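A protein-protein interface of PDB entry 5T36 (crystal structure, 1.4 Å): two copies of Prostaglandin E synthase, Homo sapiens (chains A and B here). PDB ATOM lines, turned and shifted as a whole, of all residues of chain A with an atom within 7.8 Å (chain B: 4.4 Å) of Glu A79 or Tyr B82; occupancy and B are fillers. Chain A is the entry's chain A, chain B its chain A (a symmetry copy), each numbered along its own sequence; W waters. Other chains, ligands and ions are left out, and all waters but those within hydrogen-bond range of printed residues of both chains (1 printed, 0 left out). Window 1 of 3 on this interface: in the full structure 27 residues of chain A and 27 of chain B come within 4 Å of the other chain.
O of Met A78 sits at hydrogen-bond distance from OH of Tyr B82 (2.8 Å).
OE2 of Glu A79 lies within salt-bridge range of NE of Arg A75, 2.7 Å away.
Among the printed residues, pairs that only touch across the chains: Arg A75 with His B74 (3.8 Å), Arg A75 with Met B78 (3.96 Å), Met A78 with Met B78 (3.8 Å), Glu A79 with His B74 (3.5 Å), Glu A79 with Met B78 (3.7 Å), Glu A79 with Tyr B82 (3.6 Å), Tyr A82 with Tyr B82 (3.6 Å), Pro A83 with Tyr B82 (3.3 Å) and Phe A86 with Leu B85 (3.99 Å).
Printed residues of chain B within 4 Å of Glu A79: His B74, Met B78 and Tyr B82. Of chain A, only Met A78 (2.8 Å), Glu A79 (3.6 Å), Tyr A82 (3.6 Å) and Pro A83 (3.3 Å) come within 4 Å of Tyr B82. No residue of chain A comes within 4 Å of Pro B83. Of the printed residues of chain A, His B74 touches Arg A75 and Glu A79. Printed residues of chain A within 4 Å of Met B78: Arg A75, Met A78 and Glu A79. Printed residues of chain B within 4 Å of Pro A83: Tyr B82. Of the printed residues of chain A, Leu B85 touches Phe A86 (3.99 Å). The nearest printed residue of chain B that does not touch Arg A75 is Tyr B82 (6.7 Å).
Of the 11 printed residues of chain B, 4 touch a printed residue of chain A. Printed residues of chain A that touch a printed residue of chain B: Arg A75, Met A78, Glu A79, Tyr A82, Pro A83 and Phe A86. Along chain A the printed residues that touch a printed residue of chain B span positions 75 to 86. Among the printed residues, 10 pairs touch across the chains. Among the printed residues, no Asp or Glu carboxylate lies within 4 Å of a Lys or Arg side-chain nitrogen of the other chain.
Met B78 touches its own counterpart, Met A78. Met A78 touches Tyr B82, but with the chains exchanged Tyr A82 does not touch Met B78 (5.6 Å). Tyr A82 touches its own counterpart, Tyr B82. Pro A83 touches Tyr B82, but with the chains exchanged Tyr A82 does not touch Pro B83 (8.4 Å). Positions printed for both chains: 29, 74, 77, 78, 80, 81, 82, 83, 84 and 86.
Water W1 lies within hydrogen-bond range of the backbone carbonyl oxygen (O) of Glu A79 (2.6 Å), a ring nitrogen (NE2) of His B74 (2.9 Å) and the side-chain hydroxyl (OH) of Tyr B82 (3.1 Å).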
ATOM      1  N   MET A  29       7.352 -31.151 -26.451  1.00  0.00           N
ATOM      2  CA  MET A  29       7.358 -29.823 -25.837  1.00  0.00           C
ATOM      3  C   MET A  29       8.733 -29.174 -25.945  1.00  0.00           C
ATOM      4  O   MET A  29       8.837 -27.970 -26.197  1.00  0.00           O
ATOM      5  CB  MET A  29       6.904 -29.888 -24.376  1.00  0.00           C
ATOM      6  CG  MET A  29       5.420 -30.186 -24.212  1.00  0.00           C
ATOM      7  SD  MET A  29       4.851 -30.134 -22.502  1.00  0.00           S
ATOM      8  CE  MET A  29       4.939 -28.384 -22.146  1.00  0.00           C
ATOM      9  N   ARG A  72       1.984 -19.556 -27.482  1.00  0.00           N
ATOM     10  CA  ARG A  72       0.621 -20.038 -27.229  1.00  0.00           C
ATOM     11  C   ARG A  72       0.524 -21.561 -27.306  1.00  0.00           C
ATOM     12  O   ARG A  72      -0.146 -22.185 -26.478  1.00  0.00           O
ATOM     13  CB  ARG A  72      -0.380 -19.402 -28.194  1.00  0.00           C
ATOM     14  CG  ARG A  72      -0.682 -17.943 -27.902  1.00  0.00           C
ATOM     15  CD  ARG A  72      -1.950 -17.465 -28.606  1.00  0.00           C
ATOM     16  NE  ARG A  72      -1.860 -17.504 -30.068  1.00  0.00           N
ATOM     17  CZ  ARG A  72      -1.273 -16.575 -30.818  1.00  0.00           C
ATOM     18  NH1 ARG A  72      -0.701 -15.516 -30.259  1.00  0.00           N
ATOM     19  NH2 ARG A  72      -1.253 -16.709 -32.140  1.00  0.00           N
ATOM     20  N   ALA A  73       1.189 -22.149 -28.299  1.00  0.00           N
ATOM     21  CA  ALA A  73       1.227 -23.602 -28.451  1.00  0.00           C
ATOM     22  C   ALA A  73       1.916 -24.251 -27.255  1.00  0.00           C
ATOM     23  O   ALA A  73       1.427 -25.247 -26.714  1.00  0.00           O
ATOM     24  CB  ALA A  73       1.923 -23.989 -29.745  1.00  0.00           C
ATOM     25  N   HIS A  74       3.042 -23.668 -26.843  1.00  0.00           N
ATOM     26  CA  HIS A  74       3.784 -24.142 -25.680  1.00  0.00           C
ATOM     27  C   HIS A  74       2.945 -24.027 -24.409  1.00  0.00           C
ATOM     28  O   HIS A  74       2.931 -24.952 -23.590  1.00  0.00           O
ATOM     29  CB  HIS A  74       5.092 -23.363 -25.514  1.00  0.00           C
ATOM     30  CG  HIS A  74       6.144 -24.099 -24.742  1.00  0.00           C
ATOM     31  ND1 HIS A  74       7.474 -23.738 -24.774  1.00  0.00           N
ATOM     32  CD2 HIS A  74       6.070 -25.184 -23.933  1.00  0.00           C
ATOM     33  CE1 HIS A  74       8.172 -24.559 -24.011  1.00  0.00           C
ATOM     34  NE2 HIS A  74       7.344 -25.447 -23.488  1.00  0.00           N
ATOM     35  N   ARG A  75       2.249 -22.899 -24.245  1.00  0.00           N
ATOM     36  CA  ARG A  75       1.412 -22.706 -23.068  1.00  0.00           C
ATOM     37  C   ARG A  75       0.247 -23.695 -23.045  1.00  0.00           C
ATOM     38  O   ARG A  75      -0.061 -24.261 -21.998  1.00  0.00           O
ATOM     39  CB  ARG A  75       0.909 -21.266 -22.950  1.00  0.00           C
ATOM     40  CG  ARG A  75       0.187 -21.026 -21.636  1.00  0.00           C
ATOM     41  CD  ARG A  75      -0.426 -19.655 -21.520  1.00  0.00           C
ATOM     42  NE  ARG A  75      -1.560 -19.708 -20.602  1.00  0.00           N
ATOM     43  CZ  ARG A  75      -1.934 -18.727 -19.787  1.00  0.00           C
ATOM     44  NH1 ARG A  75      -2.984 -18.904 -19.001  1.00  0.00           N
ATOM     45  NH2 ARG A  75      -1.265 -17.580 -19.747  1.00  0.00           N
ATOM     46  N   ASN A  76      -0.384 -23.915 -24.197  1.00  0.00           N
ATOM     47  CA  ASN A  76      -1.475 -24.884 -24.266  1.00  0.00           C
ATOM     48  C   ASN A  76      -0.993 -26.289 -23.906  1.00  0.00           C
ATOM     49  O   ASN A  76      -1.699 -27.031 -23.222  1.00  0.00           O
ATOM     50  CB  ASN A  76      -2.173 -24.860 -25.629  1.00  0.00           C
ATOM     51  CG  ASN A  76      -3.485 -25.622 -25.619  1.00  0.00           C
ATOM     52  OD1 ASN A  76      -3.510 -26.838 -25.804  1.00  0.00           O
ATOM     53  ND2 ASN A  76      -4.583 -24.909 -25.394  1.00  0.00           N
ATOM     54  N   ASP A  77       0.218 -26.632 -24.348  1.00  0.00           N
ATOM     55  CA  ASP A  77       0.884 -27.868 -23.930  1.00  0.00           C
ATOM     56  C   ASP A  77       0.980 -27.957 -22.405  1.00  0.00           C
ATOM     57  O   ASP A  77       0.681 -28.995 -21.822  1.00  0.00           O
ATOM     58  CB  ASP A  77       2.295 -27.958 -24.520  1.00  0.00           C
ATOM     59  CG  ASP A  77       2.312 -28.332 -25.991  1.00  0.00           C
ATOM     60  OD1 ASP A  77       1.242 -28.546 -26.601  1.00  0.00           O
ATOM     61  OD2 ASP A  77       3.430 -28.411 -26.538  1.00  0.00           O
ATOM     62  N   MET A  78       1.400 -26.867 -21.765  1.00  0.00           N
ATOM     63  CA  MET A  78       1.516 -26.831 -20.304  1.00  0.00           C
ATOM     64  C   MET A  78       0.156 -26.971 -19.619  1.00  0.00           C
ATOM     65  O   MET A  78       0.055 -27.553 -18.538  1.00  0.00           O
ATOM     66  CB  MET A  78       2.222 -25.556 -19.837  1.00  0.00           C
ATOM     67  CG  MET A  78       3.670 -25.449 -20.290  1.00  0.00           C
ATOM     68  SD  MET A  78       4.628 -24.264 -19.331  1.00  0.00           S
ATOM     69  CE  MET A  78       4.061 -22.711 -20.026  1.00  0.00           C
ATOM     70  N   GLU A  79      -0.884 -26.449 -20.265  1.00  0.00           N
ATOM     71  CA  GLU A  79      -2.249 -26.520 -19.742  1.00  0.00           C
ATOM     72  C   GLU A  79      -2.875 -27.914 -19.869  1.00  0.00           C
ATOM     73  O   GLU A  79      -3.886 -28.202 -19.222  1.00  0.00           O
ATOM     74  CB  GLU A  79      -3.140 -25.475 -20.430  1.00  0.00           C
ATOM     75  CG  GLU A  79      -2.774 -24.026 -20.093  1.00  0.00           C
ATOM     76  CD  GLU A  79      -3.531 -22.988 -20.914  1.00  0.00           C
ATOM     77  OE1 GLU A  79      -4.312 -23.363 -21.813  1.00  0.00           O
ATOM     78  OE2 GLU A  79      -3.333 -21.782 -20.656  1.00  0.00           O
ATOM     79  N   THR A  80      -2.273 -28.777 -20.688  1.00  0.00           N
ATOM     80  CA  THR A  80      -2.881 -30.071 -21.023  1.00  0.00           C
ATOM     81  C   THR A  80      -1.978 -31.283 -20.795  1.00  0.00           C
ATOM     82  O   THR A  80      -2.414 -32.281 -20.214  1.00  0.00           O
ATOM     83  CB  THR A  80      -3.375 -30.104 -22.484  1.00  0.00           C
ATOM     84  OG1 THR A  80      -2.292 -29.772 -23.359  1.00  0.00           O
ATOM     85  CG2 THR A  80      -4.519 -29.118 -22.694  1.00  0.00           C
ATOM     86  N   ILE A  81      -0.734 -31.202 -21.262  1.00  0.00           N
ATOM     87  CA  ILE A  81       0.207 -32.318 -21.140  1.00  0.00           C
ATOM     88  C   ILE A  81       0.636 -32.539 -19.687  1.00  0.00           C
ATOM     89  O   ILE A  81       0.730 -33.682 -19.239  1.00  0.00           O
ATOM     90  CB  ILE A  81       1.428 -32.164 -22.091  1.00  0.00           C
ATOM     91  CG1 ILE A  81       0.960 -32.233 -23.551  1.00  0.00           C
ATOM     92  CG2 ILE A  81       2.491 -33.232 -21.803  1.00  0.00           C
ATOM     93  CD1 ILE A  81       2.003 -31.825 -24.575  1.00  0.00           C
ATOM     94  N   TYR A  82       0.883 -31.456 -18.951  1.00  0.00           N
ATOM     95  CA  TYR A  82       1.275 -31.586 -17.543  1.00  0.00           C
ATOM     96  C   TYR A  82       0.222 -32.319 -16.689  1.00  0.00           C
ATOM     97  O   TYR A  82       0.582 -33.224 -15.936  1.00  0.00           O
ATOM     98  CB  TYR A  82       1.676 -30.239 -16.915  1.00  0.00           C
ATOM     99  CG  TYR A  82       2.932 -29.596 -17.485  1.00  0.00           C
ATOM    100  CD1 TYR A  82       3.840 -30.323 -18.263  1.00  0.00           C
ATOM    101  CD2 TYR A  82       3.226 -28.260 -17.215  1.00  0.00           C
ATOM    102  CE1 TYR A  82       4.990 -29.725 -18.774  1.00  0.00           C
ATOM    103  CE2 TYR A  82       4.375 -27.657 -17.716  1.00  0.00           C
ATOM    104  CZ  TYR A  82       5.251 -28.393 -18.496  1.00  0.00           C
ATOM    105  OH  TYR A  82       6.386 -27.792 -18.995  1.00  0.00           O
ATOM    106  N   PRO A  83      -1.075 -31.947 -16.807  1.00  0.00           N
ATOM    107  CA  PRO A  83      -2.112 -32.730 -16.122  1.00  0.00           C
ATOM    108  C   PRO A  83      -2.128 -34.207 -16.525  1.00  0.00           C
ATOM    109  O   PRO A  83      -2.354 -35.069 -15.673  1.00  0.00           O
ATOM    110  CB  PRO A  83      -3.411 -32.055 -16.565  1.00  0.00           C
ATOM    111  CG  PRO A  83      -3.029 -30.659 -16.831  1.00  0.00           C
ATOM    112  CD  PRO A  83      -1.630 -30.700 -17.373  1.00  0.00           C
ATOM    113  N   PHE A  84      -1.894 -34.490 -17.807  1.00  0.00           N
ATOM    114  CA  PHE A  84      -1.829 -35.869 -18.301  1.00  0.00           C
ATOM    115  C   PHE A  84      -0.711 -36.670 -17.636  1.00  0.00           C
ATOM    116  O   PHE A  84      -0.893 -37.850 -17.326  1.00  0.00           O
ATOM    117  CB  PHE A  84      -1.669 -35.895 -19.824  1.00  0.00           C
ATOM    118  CG  PHE A  84      -1.440 -37.271 -20.397  1.00  0.00           C
ATOM    119  CD1 PHE A  84      -2.511 -38.122 -20.652  1.00  0.00           C
ATOM    120  CD2 PHE A  84      -0.152 -37.711 -20.696  1.00  0.00           C
ATOM    121  CE1 PHE A  84      -2.304 -39.394 -21.187  1.00  0.00           C
ATOM    122  CE2 PHE A  84       0.066 -38.981 -21.229  1.00  0.00           C
ATOM    123  CZ  PHE A  84      -1.012 -39.822 -21.475  1.00  0.00           C
ATOM    124  N   PHE A  86       0.370 -36.399 -14.677  1.00  0.00           N
ATOM    125  CA  PHE A  86      -0.140 -36.795 -13.370  1.00  0.00           C
ATOM    126  C   PHE A  86      -1.248 -37.846 -13.482  1.00  0.00           C
ATOM    127  O   PHE A  86      -1.150 -38.920 -12.881  1.00  0.00           O
ATOM    128  CB  PHE A  86      -0.634 -35.574 -12.585  1.00  0.00           C
ATOM    129  CG  PHE A  86      -1.244 -35.918 -11.255  1.00  0.00           C
ATOM    130  CD1 PHE A  86      -0.436 -36.221 -10.162  1.00  0.00           C
ATOM    131  CD2 PHE A  86      -2.626 -35.954 -11.098  1.00  0.00           C
ATOM    132  CE1 PHE A  86      -0.993 -36.550  -8.932  1.00  0.00           C
ATOM    133  CE2 PHE A  86      -3.195 -36.282  -9.869  1.00  0.00           C
ATOM    134  CZ  PHE A  86      -2.374 -36.581  -8.786  1.00  0.00           C
ATOM    135  N   PHE A 108      -4.588 -39.404 -26.610  1.00  0.00           N
ATOM    136  CA  PHE A 108      -3.941 -38.187 -26.122  1.00  0.00           C
ATOM    137  C   PHE A 108      -2.688 -37.841 -26.923  1.00  0.00           C
ATOM    138  O   PHE A 108      -2.505 -36.689 -27.315  1.00  0.00           O
ATOM    139  CB  PHE A 108      -3.612 -38.265 -24.628  1.00  0.00           C
ATOM    140  CG  PHE A 108      -3.193 -36.944 -24.041  1.00  0.00           C
ATOM    141  CD1 PHE A 108      -4.136 -35.952 -23.798  1.00  0.00           C
ATOM    142  CD2 PHE A 108      -1.858 -36.679 -23.760  1.00  0.00           C
ATOM    143  CE1 PHE A 108      -3.763 -34.720 -23.270  1.00  0.00           C
ATOM    144  CE2 PHE A 108      -1.473 -35.445 -23.229  1.00  0.00           C
ATOM    145  CZ  PHE A 108      -2.430 -34.467 -22.982  1.00  0.00           C
ATOM    146  N   ARG A 112      -2.586 -34.541 -29.237  1.00  0.00           N
ATOM    147  CA  ARG A 112      -1.650 -33.468 -28.888  1.00  0.00           C
ATOM    148  C   ARG A 112      -0.611 -33.170 -29.970  1.00  0.00           C
ATOM    149  O   ARG A 112      -0.268 -32.009 -30.193  1.00  0.00           O
ATOM    150  CB  ARG A 112      -0.960 -33.745 -27.549  1.00  0.00           C
ATOM    151  CG  ARG A 112      -1.867 -33.645 -26.319  1.00  0.00           C
ATOM    152  CD  ARG A 112      -2.728 -32.380 -26.289  1.00  0.00           C
ATOM    153  NE  ARG A 112      -1.947 -31.146 -26.375  1.00  0.00           N
ATOM    154  CZ  ARG A 112      -2.469 -29.923 -26.317  1.00  0.00           C
ATOM    155  NH1 ARG A 112      -3.777 -29.754 -26.160  1.00  0.00           N
ATOM    156  NH2 ARG A 112      -1.676 -28.863 -26.402  1.00  0.00           N
ATOM    157  N   TYR A 132      -7.708 -30.433 -29.627  1.00  0.00           N
ATOM    158  CA  TYR A 132      -7.701 -30.139 -28.194  1.00  0.00           C
ATOM    159  C   TYR A 132      -8.771 -30.952 -27.469  1.00  0.00           C
ATOM    160  O   TYR A 132      -8.485 -31.619 -26.472  1.00  0.00           O
ATOM    161  CB  TYR A 132      -7.919 -28.642 -27.939  1.00  0.00           C
ATOM    162  CG  TYR A 132      -8.240 -28.311 -26.495  1.00  0.00           C
ATOM    163  CD1 TYR A 132      -7.225 -28.182 -25.547  1.00  0.00           C
ATOM    164  CD2 TYR A 132      -9.561 -28.139 -26.072  1.00  0.00           C
ATOM    165  CE1 TYR A 132      -7.515 -27.887 -24.220  1.00  0.00           C
ATOM    166  CE2 TYR A 132      -9.860 -27.844 -24.743  1.00  0.00           C
ATOM    167  CZ  TYR A 132      -8.831 -27.720 -23.825  1.00  0.00           C
ATOM    168  OH  TYR A 132      -9.114 -27.428 -22.510  1.00  0.00           O
ATOM    169  N   GLN A 136      -8.548 -34.073 -24.741  1.00  0.00           N
ATOM    170  CA  GLN A 136      -9.091 -33.880 -23.394  1.00  0.00           C
ATOM    171  C   GLN A 136     -10.005 -35.021 -22.949  1.00  0.00           C
ATOM    172  O   GLN A 136     -10.139 -35.275 -21.750  1.00  0.00           O
ATOM    173  CB  GLN A 136      -9.821 -32.536 -23.273  1.00  0.00           C
ATOM    174  CG  GLN A 136      -8.904 -31.316 -23.264  1.00  0.00           C
ATOM    175  CD  GLN A 136      -7.860 -31.370 -22.163  1.00  0.00           C
ATOM    176  OE1 GLN A 136      -6.734 -31.813 -22.385  1.00  0.00           O
ATOM    177  NE2 GLN A 136      -8.237 -30.932 -20.966  1.00  0.00           N
ATOM    178  N   MET B  29      -9.138 -26.955 -13.035  1.00  0.00           N
ATOM    179  CA  MET B  29      -8.338 -26.295 -14.066  1.00  0.00           C
ATOM    180  C   MET B  29      -8.954 -26.487 -15.447  1.00  0.00           C
ATOM    181  O   MET B  29      -8.964 -25.560 -16.261  1.00  0.00           O
ATOM    182  CB  MET B  29      -6.890 -26.793 -14.045  1.00  0.00           C
ATOM    183  CG  MET B  29      -6.100 -26.320 -12.834  1.00  0.00           C
ATOM    184  SD  MET B  29      -4.360 -26.793 -12.867  1.00  0.00           S
ATOM    185  CE  MET B  29      -3.730 -25.751 -14.176  1.00  0.00           C
ATOM    186  N   HIS B  74      -5.814 -19.186 -14.857  1.00  0.00           N
ATOM    187  CA  HIS B  74      -5.283 -20.455 -15.342  1.00  0.00           C
ATOM    188  C   HIS B  74      -3.773 -20.537 -15.123  1.00  0.00           C
ATOM    189  O   HIS B  74      -3.265 -21.577 -14.692  1.00  0.00           O
ATOM    190  CB  HIS B  74      -5.605 -20.649 -16.826  1.00  0.00           C
ATOM    191  CG  HIS B  74      -5.611 -22.082 -17.266  1.00  0.00           C
ATOM    192  ND1 HIS B  74      -6.201 -22.492 -18.441  1.00  0.00           N
ATOM    193  CD2 HIS B  74      -5.117 -23.201 -16.683  1.00  0.00           C
ATOM    194  CE1 HIS B  74      -6.061 -23.799 -18.570  1.00  0.00           C
ATOM    195  NE2 HIS B  74      -5.407 -24.255 -17.516  1.00  0.00           N
ATOM    196  N   ASP B  77      -2.961 -21.028 -11.473  1.00  0.00           N
ATOM    197  CA  ASP B  77      -3.187 -22.453 -11.222  1.00  0.00           C
ATOM    198  C   ASP B  77      -1.956 -23.283 -11.591  1.00  0.00           C
ATOM    199  O   ASP B  77      -1.534 -24.147 -10.827  1.00  0.00           O
ATOM    200  CB  ASP B  77      -4.387 -22.968 -12.024  1.00  0.00           C
ATOM    201  CG  ASP B  77      -5.726 -22.553 -11.441  1.00  0.00           C
ATOM    202  OD1 ASP B  77      -5.775 -21.869 -10.396  1.00  0.00           O
ATOM    203  OD2 ASP B  77      -6.746 -22.929 -12.053  1.00  0.00           O
ATOM    204  N   MET B  78      -1.382 -23.019 -12.764  1.00  0.00           N
ATOM    205  CA  MET B  78      -0.188 -23.739 -13.214  1.00  0.00           C
ATOM    206  C   MET B  78       1.020 -23.461 -12.318  1.00  0.00           C
ATOM    207  O   MET B  78       1.865 -24.334 -12.115  1.00  0.00           O
ATOM    208  CB  MET B  78       0.140 -23.408 -14.672  1.00  0.00           C
ATOM    209  CG  MET B  78      -0.919 -23.865 -15.664  1.00  0.00           C
ATOM    210  SD  MET B  78      -0.312 -23.960 -17.356  1.00  0.00           S
ATOM    211  CE  MET B  78      -0.303 -22.228 -17.822  1.00  0.00           C
ATOM    212  N   THR B  80       0.897 -23.001  -9.143  1.00  0.00           N
ATOM    213  CA  THR B  80       0.630 -23.458  -7.774  1.00  0.00           C
ATOM    214  C   THR B  80       0.133 -24.899  -7.663  1.00  0.00           C
ATOM    215  O   THR B  80       0.626 -25.663  -6.827  1.00  0.00           O
ATOM    216  CB  THR B  80      -0.381 -22.540  -7.057  1.00  0.00           C
ATOM    217  OG1 THR B  80      -1.577 -22.450  -7.839  1.00  0.00           O
ATOM    218  CG2 THR B  80       0.199 -21.145  -6.851  1.00  0.00           C
ATOM    219  N   ILE B  81      -0.845 -25.263  -8.489  1.00  0.00           N
ATOM    220  CA  ILE B  81      -1.430 -26.605  -8.443  1.00  0.00           C
ATOM    221  C   ILE B  81      -0.448 -27.667  -8.943  1.00  0.00           C
ATOM    222  O   ILE B  81      -0.353 -28.745  -8.357  1.00  0.00           O
ATOM    223  CB  ILE B  81      -2.793 -26.677  -9.187  1.00  0.00           C
ATOM    224  CG1 ILE B  81      -3.826 -25.800  -8.466  1.00  0.00           C
ATOM    225  CG2 ILE B  81      -3.286 -28.126  -9.300  1.00  0.00           C
ATOM    226  CD1 ILE B  81      -5.113 -25.563  -9.235  1.00  0.00           C
ATOM    227  N   TYR B  82       0.289 -27.364 -10.012  1.00  0.00           N
ATOM    228  CA  TYR B  82       1.270 -28.321 -10.535  1.00  0.00           C
ATOM    229  C   TYR B  82       2.348 -28.704  -9.502  1.00  0.00           C
ATOM    230  O   TYR B  82       2.624 -29.892  -9.334  1.00  0.00           O
ATOM    231  CB  TYR B  82       1.898 -27.856 -11.862  1.00  0.00           C
ATOM    232  CG  TYR B  82       0.944 -27.775 -13.045  1.00  0.00           C
ATOM    233  CD1 TYR B  82      -0.308 -28.399 -13.024  1.00  0.00           C
ATOM    234  CD2 TYR B  82       1.316 -27.096 -14.206  1.00  0.00           C
ATOM    235  CE1 TYR B  82      -1.170 -28.322 -14.116  1.00  0.00           C
ATOM    236  CE2 TYR B  82       0.465 -27.021 -15.303  1.00  0.00           C
ATOM    237  CZ  TYR B  82      -0.776 -27.632 -15.252  1.00  0.00           C
ATOM    238  OH  TYR B  82      -1.619 -27.552 -16.339  1.00  0.00           O
ATOM    239  N   PRO B  83       2.951 -27.713  -8.802  1.00  0.00           N
ATOM    240  CA  PRO B  83       3.867 -28.063  -7.708  1.00  0.00           C
ATOM    241  C   PRO B  83       3.218 -28.923  -6.619  1.00  0.00           C
ATOM    242  O   PRO B  83       3.871 -29.825  -6.087  1.00  0.00           O
ATOM    243  CB  PRO B  83       4.258 -26.701  -7.130  1.00  0.00           C
ATOM    244  CG  PRO B  83       4.144 -25.773  -8.266  1.00  0.00           C
ATOM    245  CD  PRO B  83       3.001 -26.268  -9.103  1.00  0.00           C
ATOM    246  N   PHE B  84       1.956 -28.645  -6.296  1.00  0.00           N
ATOM    247  CA  PHE B  84       1.213 -29.434  -5.309  1.00  0.00           C
ATOM    248  C   PHE B  84       1.071 -30.897  -5.727  1.00  0.00           C
ATOM    249  O   PHE B  84       1.172 -31.795  -4.887  1.00  0.00           O
ATOM    250  CB  PHE B  84      -0.165 -28.820  -5.047  1.00  0.00           C
ATOM    251  CG  PHE B  84      -1.054 -29.656  -4.160  1.00  0.00           C
ATOM    252  CD1 PHE B  84      -0.936 -29.593  -2.774  1.00  0.00           C
ATOM    253  CD2 PHE B  84      -2.022 -30.494  -4.711  1.00  0.00           C
ATOM    254  CE1 PHE B  84      -1.761 -30.361  -1.950  1.00  0.00           C
ATOM    255  CE2 PHE B  84      -2.850 -31.266  -3.895  1.00  0.00           C
ATOM    256  CZ  PHE B  84      -2.718 -31.198  -2.514  1.00  0.00           C
ATOM    257  N   LEU B  85       0.834 -31.129  -7.020  1.00  0.00           N
ATOM    258  CA  LEU B  85       0.713 -32.486  -7.558  1.00  0.00           C
ATOM    259  C   LEU B  85       1.970 -33.302  -7.270  1.00  0.00           C
ATOM    260  O   LEU B  85       1.888 -34.488  -6.952  1.00  0.00           O
ATOM    261  CB  LEU B  85       0.428 -32.468  -9.066  1.00  0.00           C
ATOM    262  CG  LEU B  85      -0.853 -31.805  -9.588  1.00  0.00           C
ATOM    263  CD1 LEU B  85      -0.904 -31.882 -11.103  1.00  0.00           C
ATOM    264  CD2 LEU B  85      -2.101 -32.427  -8.989  1.00  0.00           C
ATOM    265  N   PHE B  86       3.126 -32.651  -7.372  1.00  0.00           N
ATOM    266  CA  PHE B  86       4.398 -33.285  -7.053  1.00  0.00           C
ATOM    267  C   PHE B  86       4.614 -33.415  -5.544  1.00  0.00           C
ATOM    268  O   PHE B  86       4.850 -34.517  -5.041  1.00  0.00           O
ATOM    269  CB  PHE B  86       5.563 -32.524  -7.700  1.00  0.00           C
ATOM    270  CG  PHE B  86       6.915 -33.082  -7.352  1.00  0.00           C
ATOM    271  CD1 PHE B  86       7.392 -34.228  -7.982  1.00  0.00           C
ATOM    272  CD2 PHE B  86       7.706 -32.469  -6.386  1.00  0.00           C
ATOM    273  CE1 PHE B  86       8.637 -34.755  -7.658  1.00  0.00           C
ATOM    274  CE2 PHE B  86       8.955 -32.988  -6.054  1.00  0.00           C
ATOM    275  CZ  PHE B  86       9.419 -34.134  -6.692  1.00  0.00           C
HETATM  276  O   HOH W   1      -4.616 -27.005 -17.004  1.00  0.00           O
